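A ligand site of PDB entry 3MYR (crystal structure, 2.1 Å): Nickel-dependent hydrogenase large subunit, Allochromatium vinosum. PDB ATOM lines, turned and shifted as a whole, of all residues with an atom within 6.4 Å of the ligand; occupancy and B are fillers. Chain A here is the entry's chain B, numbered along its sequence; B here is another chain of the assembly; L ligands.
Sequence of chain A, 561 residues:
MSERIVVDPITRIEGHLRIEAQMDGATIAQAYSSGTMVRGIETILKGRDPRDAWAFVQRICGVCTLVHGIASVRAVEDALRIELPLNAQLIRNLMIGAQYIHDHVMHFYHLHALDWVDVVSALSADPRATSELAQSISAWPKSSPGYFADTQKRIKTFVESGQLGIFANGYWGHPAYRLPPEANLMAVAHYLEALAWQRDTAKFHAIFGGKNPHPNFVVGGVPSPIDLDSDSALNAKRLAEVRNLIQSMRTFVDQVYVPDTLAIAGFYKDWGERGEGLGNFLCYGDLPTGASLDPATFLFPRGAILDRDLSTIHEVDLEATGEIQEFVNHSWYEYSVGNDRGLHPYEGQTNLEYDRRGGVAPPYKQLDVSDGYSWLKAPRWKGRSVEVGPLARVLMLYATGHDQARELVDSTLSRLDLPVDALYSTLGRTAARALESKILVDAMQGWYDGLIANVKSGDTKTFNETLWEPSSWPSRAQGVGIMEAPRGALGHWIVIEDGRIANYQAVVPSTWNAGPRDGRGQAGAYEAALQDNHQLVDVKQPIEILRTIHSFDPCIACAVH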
ATOM      1  N   GLU A  14     -33.097 -31.852  23.650  1.00  0.00           N
ATOM      2  CA  GLU A  14     -32.889 -31.121  24.915  1.00  0.00           C
ATOM      3  C   GLU A  14     -34.210 -30.465  25.332  1.00  0.00           C
ATOM      4  O   GLU A  14     -34.885 -29.831  24.514  1.00  0.00           O
ATOM      5  CB  GLU A  14     -31.833 -30.032  24.708  1.00  0.00           C
ATOM      6  CG  GLU A  14     -31.352 -29.405  26.078  1.00  0.00           C
ATOM      7  CD  GLU A  14     -32.487 -28.675  26.846  1.00  0.00           C
ATOM      8  OE1 GLU A  14     -32.505 -28.779  28.135  1.00  0.00           O
ATOM      9  OE2 GLU A  14     -33.346 -28.014  26.167  1.00  0.00           O
ATOM     10  N   ILE A  60     -28.759 -20.724  29.966  1.00  0.00           N
ATOM     11  CA  ILE A  60     -29.916 -21.074  29.146  1.00  0.00           C
ATOM     12  C   ILE A  60     -29.827 -22.522  28.712  1.00  0.00           C
ATOM     13  O   ILE A  60     -30.835 -23.241  28.652  1.00  0.00           O
ATOM     14  CB  ILE A  60     -30.034 -20.116  27.913  1.00  0.00           C
ATOM     15  CG1 ILE A  60     -30.557 -18.767  28.465  1.00  0.00           C
ATOM     16  CG2 ILE A  60     -30.980 -20.735  26.817  1.00  0.00           C
ATOM     17  CD1 ILE A  60     -30.534 -17.595  27.331  1.00  0.00           C
ATOM     18  N   CYS A  61     -28.618 -22.991  28.380  1.00  0.00           N
ATOM     19  CA  CYS A  61     -28.555 -24.337  27.820  1.00  0.00           C
ATOM     20  C   CYS A  61     -27.168 -24.915  27.867  1.00  0.00           C
ATOM     21  O   CYS A  61     -26.227 -24.255  27.501  1.00  0.00           O
ATOM     22  CB  CYS A  61     -29.100 -24.390  26.386  1.00  0.00           C
ATOM     23  SG  CYS A  61     -29.278 -26.129  25.845  1.00  0.00           S
ATOM     24  N   GLY A  62     -27.056 -26.132  28.369  1.00  0.00           N
ATOM     25  CA  GLY A  62     -25.773 -26.772  28.456  1.00  0.00           C
ATOM     26  C   GLY A  62     -25.474 -27.763  27.337  1.00  0.00           C
ATOM     27  O   GLY A  62     -24.411 -28.403  27.334  1.00  0.00           O
ATOM     28  N   VAL A  63     -26.392 -27.917  26.375  1.00  0.00           N
ATOM     29  CA  VAL A  63     -26.092 -28.767  25.194  1.00  0.00           C
ATOM     30  C   VAL A  63     -25.399 -27.860  24.187  1.00  0.00           C
ATOM     31  O   VAL A  63     -24.269 -28.124  23.805  1.00  0.00           O
ATOM     32  CB  VAL A  63     -27.366 -29.354  24.541  1.00  0.00           C
ATOM     33  CG1 VAL A  63     -26.972 -30.106  23.224  1.00  0.00           C
ATOM     34  CG2 VAL A  63     -27.958 -30.309  25.494  1.00  0.00           C
ATOM     35  N   CYS A  64     -26.024 -26.741  23.783  1.00  0.00           N
ATOM     36  CA  CYS A  64     -25.253 -25.752  23.066  1.00  0.00           C
ATOM     37  C   CYS A  64     -24.572 -24.871  24.165  1.00  0.00           C
ATOM     38  O   CYS A  64     -24.819 -23.670  24.272  1.00  0.00           O
ATOM     39  CB  CYS A  64     -26.087 -24.896  22.096  1.00  0.00           C
ATOM     40  SG  CYS A  64     -27.499 -24.120  23.010  1.00  0.00           S
ATOM     41  N   THR A  65     -23.728 -25.471  24.977  1.00  0.00           N
ATOM     42  CA  THR A  65     -22.967 -24.673  25.926  1.00  0.00           C
ATOM     43  C   THR A  65     -22.062 -23.741  25.035  1.00  0.00           C
ATOM     44  O   THR A  65     -22.047 -23.943  23.811  1.00  0.00           O
ATOM     45  CB  THR A  65     -22.126 -25.559  26.840  1.00  0.00           C
ATOM     46  OG1 THR A  65     -21.543 -24.711  27.834  1.00  0.00           O
ATOM     47  CG2 THR A  65     -21.054 -26.297  26.073  1.00  0.00           C
ATOM     48  N   VAL A  67     -22.542 -21.097  23.394  1.00  0.00           N
ATOM     49  CA  VAL A  67     -23.054 -20.169  22.350  1.00  0.00           C
ATOM     50  C   VAL A  67     -23.771 -18.937  22.930  1.00  0.00           C
ATOM     51  O   VAL A  67     -23.646 -17.858  22.356  1.00  0.00           O
ATOM     52  CB  VAL A  67     -24.026 -20.838  21.302  1.00  0.00           C
ATOM     53  CG1 VAL A  67     -23.309 -22.078  20.672  1.00  0.00           C
ATOM     54  CG2 VAL A  67     -25.342 -21.220  22.003  1.00  0.00           C
ATOM     55  N   HIS A  68     -24.460 -19.079  24.078  1.00  0.00           N
ATOM     56  CA  HIS A  68     -25.027 -17.888  24.683  1.00  0.00           C
ATOM     57  C   HIS A  68     -23.960 -17.031  25.379  1.00  0.00           C
ATOM     58  O   HIS A  68     -24.211 -15.868  25.563  1.00  0.00           O
ATOM     59  CB  HIS A  68     -26.156 -18.265  25.666  1.00  0.00           C
ATOM     60  CG  HIS A  68     -27.352 -18.876  24.975  1.00  0.00           C
ATOM     61  ND1 HIS A  68     -28.256 -18.135  24.264  1.00  0.00           N
ATOM     62  CD2 HIS A  68     -27.774 -20.164  24.884  1.00  0.00           C
ATOM     63  CE1 HIS A  68     -29.168 -18.935  23.720  1.00  0.00           C
ATOM     64  NE2 HIS A  68     -28.908 -20.172  24.094  1.00  0.00           N
ATOM     65  N   ASP A 103     -21.197 -31.015  19.190  1.00  0.00           N
ATOM     66  CA  ASP A 103     -22.647 -30.986  19.315  1.00  0.00           C
ATOM     67  C   ASP A 103     -23.334 -31.755  18.109  1.00  0.00           C
ATOM     68  O   ASP A 103     -24.193 -32.584  18.327  1.00  0.00           O
ATOM     69  CB  ASP A 103     -23.025 -29.500  19.300  1.00  0.00           C
ATOM     70  CG  ASP A 103     -24.424 -29.223  19.743  1.00  0.00           C
ATOM     71  OD1 ASP A 103     -25.328 -30.108  19.596  1.00  0.00           O
ATOM     72  OD2 ASP A 103     -24.636 -28.073  20.272  1.00  0.00           O
ATOM     73  N   ALA A 485     -25.339 -20.385  16.027  1.00  0.00           N
ATOM     74  CA  ALA A 485     -25.176 -21.480  16.997  1.00  0.00           C
ATOM     75  C   ALA A 485     -25.414 -22.787  16.200  1.00  0.00           C
ATOM     76  O   ALA A 485     -25.953 -22.727  15.093  1.00  0.00           O
ATOM     77  CB  ALA A 485     -26.224 -21.319  18.111  1.00  0.00           C
ATOM     78  N   PRO A 486     -24.950 -23.947  16.702  1.00  0.00           N
ATOM     79  CA  PRO A 486     -25.261 -25.194  15.938  1.00  0.00           C
ATOM     80  C   PRO A 486     -26.731 -25.390  15.470  1.00  0.00           C
ATOM     81  O   PRO A 486     -26.948 -25.993  14.439  1.00  0.00           O
ATOM     82  CB  PRO A 486     -24.877 -26.331  16.912  1.00  0.00           C
ATOM     83  CG  PRO A 486     -23.773 -25.683  17.730  1.00  0.00           C
ATOM     84  CD  PRO A 486     -24.232 -24.248  17.976  1.00  0.00           C
ATOM     85  N   ARG A 487     -27.711 -24.865  16.217  1.00  0.00           N
ATOM     86  CA  ARG A 487     -29.092 -24.959  15.785  1.00  0.00           C
ATOM     87  C   ARG A 487     -29.582 -23.803  14.919  1.00  0.00           C
ATOM     88  O   ARG A 487     -30.639 -23.892  14.342  1.00  0.00           O
ATOM     89  CB  ARG A 487     -30.024 -25.242  16.964  1.00  0.00           C
ATOM     90  CG  ARG A 487     -29.763 -26.629  17.531  1.00  0.00           C
ATOM     91  CD  ARG A 487     -30.194 -26.783  19.022  1.00  0.00           C
ATOM     92  NE  ARG A 487     -29.696 -28.108  19.468  1.00  0.00           N
ATOM     93  CZ  ARG A 487     -28.437 -28.379  19.834  1.00  0.00           C
ATOM     94  NH1 ARG A 487     -27.421 -27.473  19.896  1.00  0.00           N
ATOM     95  NH2 ARG A 487     -28.123 -29.601  20.002  1.00  0.00           N
ATOM     96  N   GLY A 488     -28.772 -22.754  14.749  1.00  0.00           N
ATOM     97  CA  GLY A 488     -29.103 -21.691  13.796  1.00  0.00           C
ATOM     98  C   GLY A 488     -28.848 -20.301  14.428  1.00  0.00           C
ATOM     99  O   GLY A 488     -28.148 -20.165  15.465  1.00  0.00           O
ATOM    100  N   ALA A 489     -29.465 -19.271  13.855  1.00  0.00           N
ATOM    101  CA  ALA A 489     -29.164 -17.881  14.133  1.00  0.00           C
ATOM    102  C   ALA A 489     -29.607 -17.512  15.537  1.00  0.00           C
ATOM    103  O   ALA A 489     -30.781 -17.649  15.827  1.00  0.00           O
ATOM    104  CB  ALA A 489     -29.943 -16.986  13.126  1.00  0.00           C
ATOM    105  N   LEU A 490     -28.722 -16.884  16.319  1.00  0.00           N
ATOM    106  CA  LEU A 490     -28.957 -16.614  17.726  1.00  0.00           C
ATOM    107  C   LEU A 490     -28.625 -15.151  17.861  1.00  0.00           C
ATOM    108  O   LEU A 490     -27.600 -14.706  17.325  1.00  0.00           O
ATOM    109  CB  LEU A 490     -27.956 -17.403  18.625  1.00  0.00           C
ATOM    110  CG  LEU A 490     -27.779 -16.944  20.092  1.00  0.00           C
ATOM    111  CD1 LEU A 490     -29.071 -17.184  20.873  1.00  0.00           C
ATOM    112  CD2 LEU A 490     -26.666 -17.781  20.826  1.00  0.00           C
ATOM    113  N   VAL A 508     -33.661 -17.153  19.966  1.00  0.00           N
ATOM    114  CA  VAL A 508     -32.756 -18.309  19.949  1.00  0.00           C
ATOM    115  C   VAL A 508     -33.176 -19.229  18.764  1.00  0.00           C
ATOM    116  O   VAL A 508     -34.348 -19.211  18.353  1.00  0.00           O
ATOM    117  CB  VAL A 508     -32.836 -19.017  21.328  1.00  0.00           C
ATOM    118  CG1 VAL A 508     -31.799 -20.100  21.431  1.00  0.00           C
ATOM    119  CG2 VAL A 508     -32.544 -17.935  22.430  1.00  0.00           C
ATOM    120  N   PRO A 509     -32.237 -19.955  18.158  1.00  0.00           N
ATOM    121  CA  PRO A 509     -32.639 -20.753  16.974  1.00  0.00           C
ATOM    122  C   PRO A 509     -33.872 -21.655  17.135  1.00  0.00           C
ATOM    123  O   PRO A 509     -34.781 -21.618  16.306  1.00  0.00           O
ATOM    124  CB  PRO A 509     -31.356 -21.533  16.596  1.00  0.00           C
ATOM    125  CG  PRO A 509     -30.349 -21.249  17.690  1.00  0.00           C
ATOM    126  CD  PRO A 509     -30.764 -19.934  18.318  1.00  0.00           C
ATOM    127  N   SER A 510     -33.983 -22.360  18.250  1.00  0.00           N
ATOM    128  CA  SER A 510     -35.139 -23.238  18.407  1.00  0.00           C
ATOM    129  C   SER A 510     -36.375 -22.400  18.725  1.00  0.00           C
ATOM    130  O   SER A 510     -37.456 -22.896  18.501  1.00  0.00           O
ATOM    131  CB  SER A 510     -34.898 -24.309  19.473  1.00  0.00           C
ATOM    132  OG  SER A 510     -33.972 -25.229  18.967  1.00  0.00           O
ATOM    133  N   THR A 511     -36.230 -21.140  19.185  1.00  0.00           N
ATOM    134  CA  THR A 511     -37.409 -20.233  19.230  1.00  0.00           C
ATOM    135  C   THR A 511     -38.003 -20.066  17.844  1.00  0.00           C
ATOM    136  O   THR A 511     -39.194 -20.275  17.650  1.00  0.00           O
ATOM    137  CB  THR A 511     -37.112 -18.826  19.870  1.00  0.00           C
ATOM    138  OG1 THR A 511     -36.272 -19.013  21.004  1.00  0.00           O
ATOM    139  CG2 THR A 511     -38.439 -18.171  20.327  1.00  0.00           C
ATOM    140  N   ASP A 553     -32.978 -30.798  15.487  1.00  0.00           N
ATOM    141  CA  ASP A 553     -32.130 -30.775  16.692  1.00  0.00           C
ATOM    142  C   ASP A 553     -32.775 -29.815  17.737  1.00  0.00           C
ATOM    143  O   ASP A 553     -32.154 -28.845  18.146  1.00  0.00           O
ATOM    144  CB  ASP A 553     -30.723 -30.287  16.248  1.00  0.00           C
ATOM    145  CG  ASP A 553     -29.622 -30.466  17.329  1.00  0.00           C
ATOM    146  OD1 ASP A 553     -28.466 -30.023  17.034  1.00  0.00           O
ATOM    147  OD2 ASP A 553     -29.890 -30.937  18.471  1.00  0.00           O
ATOM    148  N   PRO A 554     -34.021 -30.070  18.166  1.00  0.00           N
ATOM    149  CA  PRO A 554     -34.702 -29.125  19.071  1.00  0.00           C
ATOM    150  C   PRO A 554     -33.994 -28.936  20.414  1.00  0.00           C
ATOM    151  O   PRO A 554     -33.444 -29.893  20.967  1.00  0.00           O
ATOM    152  CB  PRO A 554     -36.071 -29.759  19.335  1.00  0.00           C
ATOM    153  CG  PRO A 554     -36.274 -30.777  18.203  1.00  0.00           C
ATOM    154  CD  PRO A 554     -34.890 -31.215  17.794  1.00  0.00           C
ATOM    155  N   CYS A 555     -34.045 -27.728  20.954  1.00  0.00           N
ATOM    156  CA  CYS A 555     -33.565 -27.464  22.287  1.00  0.00           C
ATOM    157  C   CYS A 555     -34.535 -26.471  22.914  1.00  0.00           C
ATOM    158  O   CYS A 555     -34.616 -25.313  22.491  1.00  0.00           O
ATOM    159  CB  CYS A 555     -32.143 -26.892  22.214  1.00  0.00           C
ATOM    160  SG  CYS A 555     -31.577 -26.540  23.928  1.00  0.00           S
ATOM    161  N   ILE A 556     -35.328 -26.929  23.886  1.00  0.00           N
ATOM    162  CA  ILE A 556     -36.477 -26.105  24.378  1.00  0.00           C
ATOM    163  C   ILE A 556     -35.978 -25.237  25.530  1.00  0.00           C
ATOM    164  O   ILE A 556     -36.564 -24.197  25.845  1.00  0.00           O
ATOM    165  CB  ILE A 556     -37.687 -26.974  24.806  1.00  0.00           C
ATOM    166  CG1 ILE A 556     -38.243 -27.825  23.591  1.00  0.00           C
ATOM    167  CG2 ILE A 556     -38.787 -26.106  25.342  1.00  0.00           C
ATOM    168  CD1 ILE A 556     -38.225 -27.172  22.190  1.00  0.00           C
ATOM    169  N   ALA A 557     -34.888 -25.653  26.172  1.00  0.00           N
ATOM    170  CA  ALA A 557     -34.329 -24.740  27.176  1.00  0.00           C
ATOM    171  C   ALA A 557     -33.801 -23.519  26.396  1.00  0.00           C
ATOM    172  O   ALA A 557     -34.106 -22.375  26.765  1.00  0.00           O
ATOM    173  CB  ALA A 557     -33.121 -25.439  27.949  1.00  0.00           C
ATOM    174  N   CYS A 558     -33.098 -23.729  25.281  1.00  0.00           N
ATOM    175  CA  CYS A 558     -32.767 -22.566  24.450  1.00  0.00           C
ATOM    176  C   CYS A 558     -34.009 -21.802  23.980  1.00  0.00           C
ATOM    177  O   CYS A 558     -34.039 -20.570  24.001  1.00  0.00           O
ATOM    178  CB  CYS A 558     -32.050 -23.019  23.188  1.00  0.00           C
ATOM    179  SG  CYS A 558     -30.298 -23.087  23.400  1.00  0.00           S
ATOM    180  N   ALA A 559     -35.008 -22.544  23.469  1.00  0.00           N
ATOM    181  CA  ALA A 559     -36.108 -21.881  22.761  1.00  0.00           C
ATOM    182  C   ALA A 559     -36.902 -20.934  23.708  1.00  0.00           C
ATOM    183  O   ALA A 559     -37.460 -19.911  23.267  1.00  0.00           O
ATOM    184  CB  ALA A 559     -37.102 -22.955  22.178  1.00  0.00           C
ATOM    185  N   CYS B  14     -30.858 -26.987  32.359  1.00  0.00           N
ATOM    186  CA  CYS B  14     -30.380 -26.516  31.064  1.00  0.00           C
ATOM    187  C   CYS B  14     -29.724 -27.704  30.315  1.00  0.00           C
ATOM    188  O   CYS B  14     -29.254 -27.543  29.197  1.00  0.00           O
ATOM    189  CB  CYS B  14     -29.371 -25.349  31.351  1.00  0.00           C
ATOM    190  SG  CYS B  14     -27.661 -25.950  31.793  1.00  0.00           S
HETATM  191 FE1  LIG L   1     -29.105 -23.611  21.439  1.00  0.00          FE
HETATM  192 NI1  LIG L   1     -29.547 -25.619  23.648  1.00  0.00          NI
HETATM  193  C1  LIG L   1     -28.823 -22.100  21.133  1.00  0.00           C
HETATM  194  O1  LIG L   1     -28.578 -20.915  20.815  1.00  0.00           O
HETATM  195  C2  LIG L   1     -28.051 -24.088  19.926  1.00  0.00           C
HETATM  196  N1  LIG L   1     -27.386 -24.358  18.991  1.00  0.00           N
HETATM  197  C3  LIG L   1     -30.701 -23.617  20.438  1.00  0.00           C
HETATM  198  N2  LIG L   1     -31.706 -23.608  19.836  1.00  0.00           N
HETATM  199  O2  LIG L   1     -29.393 -25.554  21.768  1.00  0.00           O
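A nickel atom (NI1) of the ligand is bound by the side-chain sulfur (SG) of Cys 555, 2.2 Å away.
The side-chain sulfur (SG) of Cys 61 binds a nickel atom (NI1) of the ligand, 2.3 Å away.
The side-chain sulfur (SG) of Cys 64 binds an iron atom (FE1) of the ligand (2.3 Å).
An iron atom (FE1) of the ligand is bound by the side-chain sulfur (SG) of Cys 558 (2.4 Å).
N1 of the ligand lies within hydrogen-bond range of N of Arg 487 (2.8 Å).
A nitrogen (N1) of the ligand is in hydrogen-bond range of the guanidinium group (NH1) of Arg 487 (3.2 Å).
A nitrogen (N2) of the ligand lies within hydrogen-bond range of the backbone NH of Ser 510, at 3.0 Å.
A nitrogen (N2) of the ligand lies within hydrogen-bond range of the side-chain hydroxyl of Ser 510 (2.9 Å).
An oxygen (O1) of the ligand sits at hydrogen-bond distance from a ring nitrogen (NE2) of His 68 (3.4 Å).
The side-chain hydroxyl of Ser 510 is in hydrogen-bond range of the backbone NH of Cys 555 (3.2 Å).
SG of Cys 555 sits close to OE2 of Glu 14 of chain A (3.2 Å).
The backbone NH (N) of Val 63 sits close to the side-chain sulfur (SG) of Cys 61 (3.4 Å).
The backbone carbonyl oxygen (O) of Cys 14 of chain B sits close to the side-chain sulfur (SG) of Cys 61 (3.6 Å).
The side-chain sulfur of Cys 558 lies close to a ring nitrogen (NE2) of His 68 (3.3 Å).
The guanidinium group of Arg 487 is in salt-bridge range of the side-chain carboxylate of Asp 103 (2.9 Å).
NH2 of Arg 487 lies within salt-bridge range of OD2 of Asp 553 (2.7 Å).
The backbone carbonyl oxygen (O) of Val 508 lies close to the side-chain hydroxyl (OG1) of Thr 511 (3.3 Å).
N1 of the ligand sits close to N of Pro 486, at 3.4 Å.
Val 67 touches the ligand (CG2 to O1, 3.5 Å).
CB of Ala 485 touches N1 of the ligand (3.4 Å).
CD2 of Leu 490 touches O1 of the ligand, at 3.7 Å.
CG1 of Val 508 touches O1 of the ligand, 3.4 Å away.
Pro 509 touches the ligand.
Within 4 Å of the ligand: Cys 61, Cys 64, Val 67, His 68, Ala 485, Pro 486, Arg 487, Leu 490, Val 508, Pro 509, Ser 510, Cys 555 and Cys 558.
The nearest printed residue that does not touch the ligand is Val 63 (4.4 Å).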
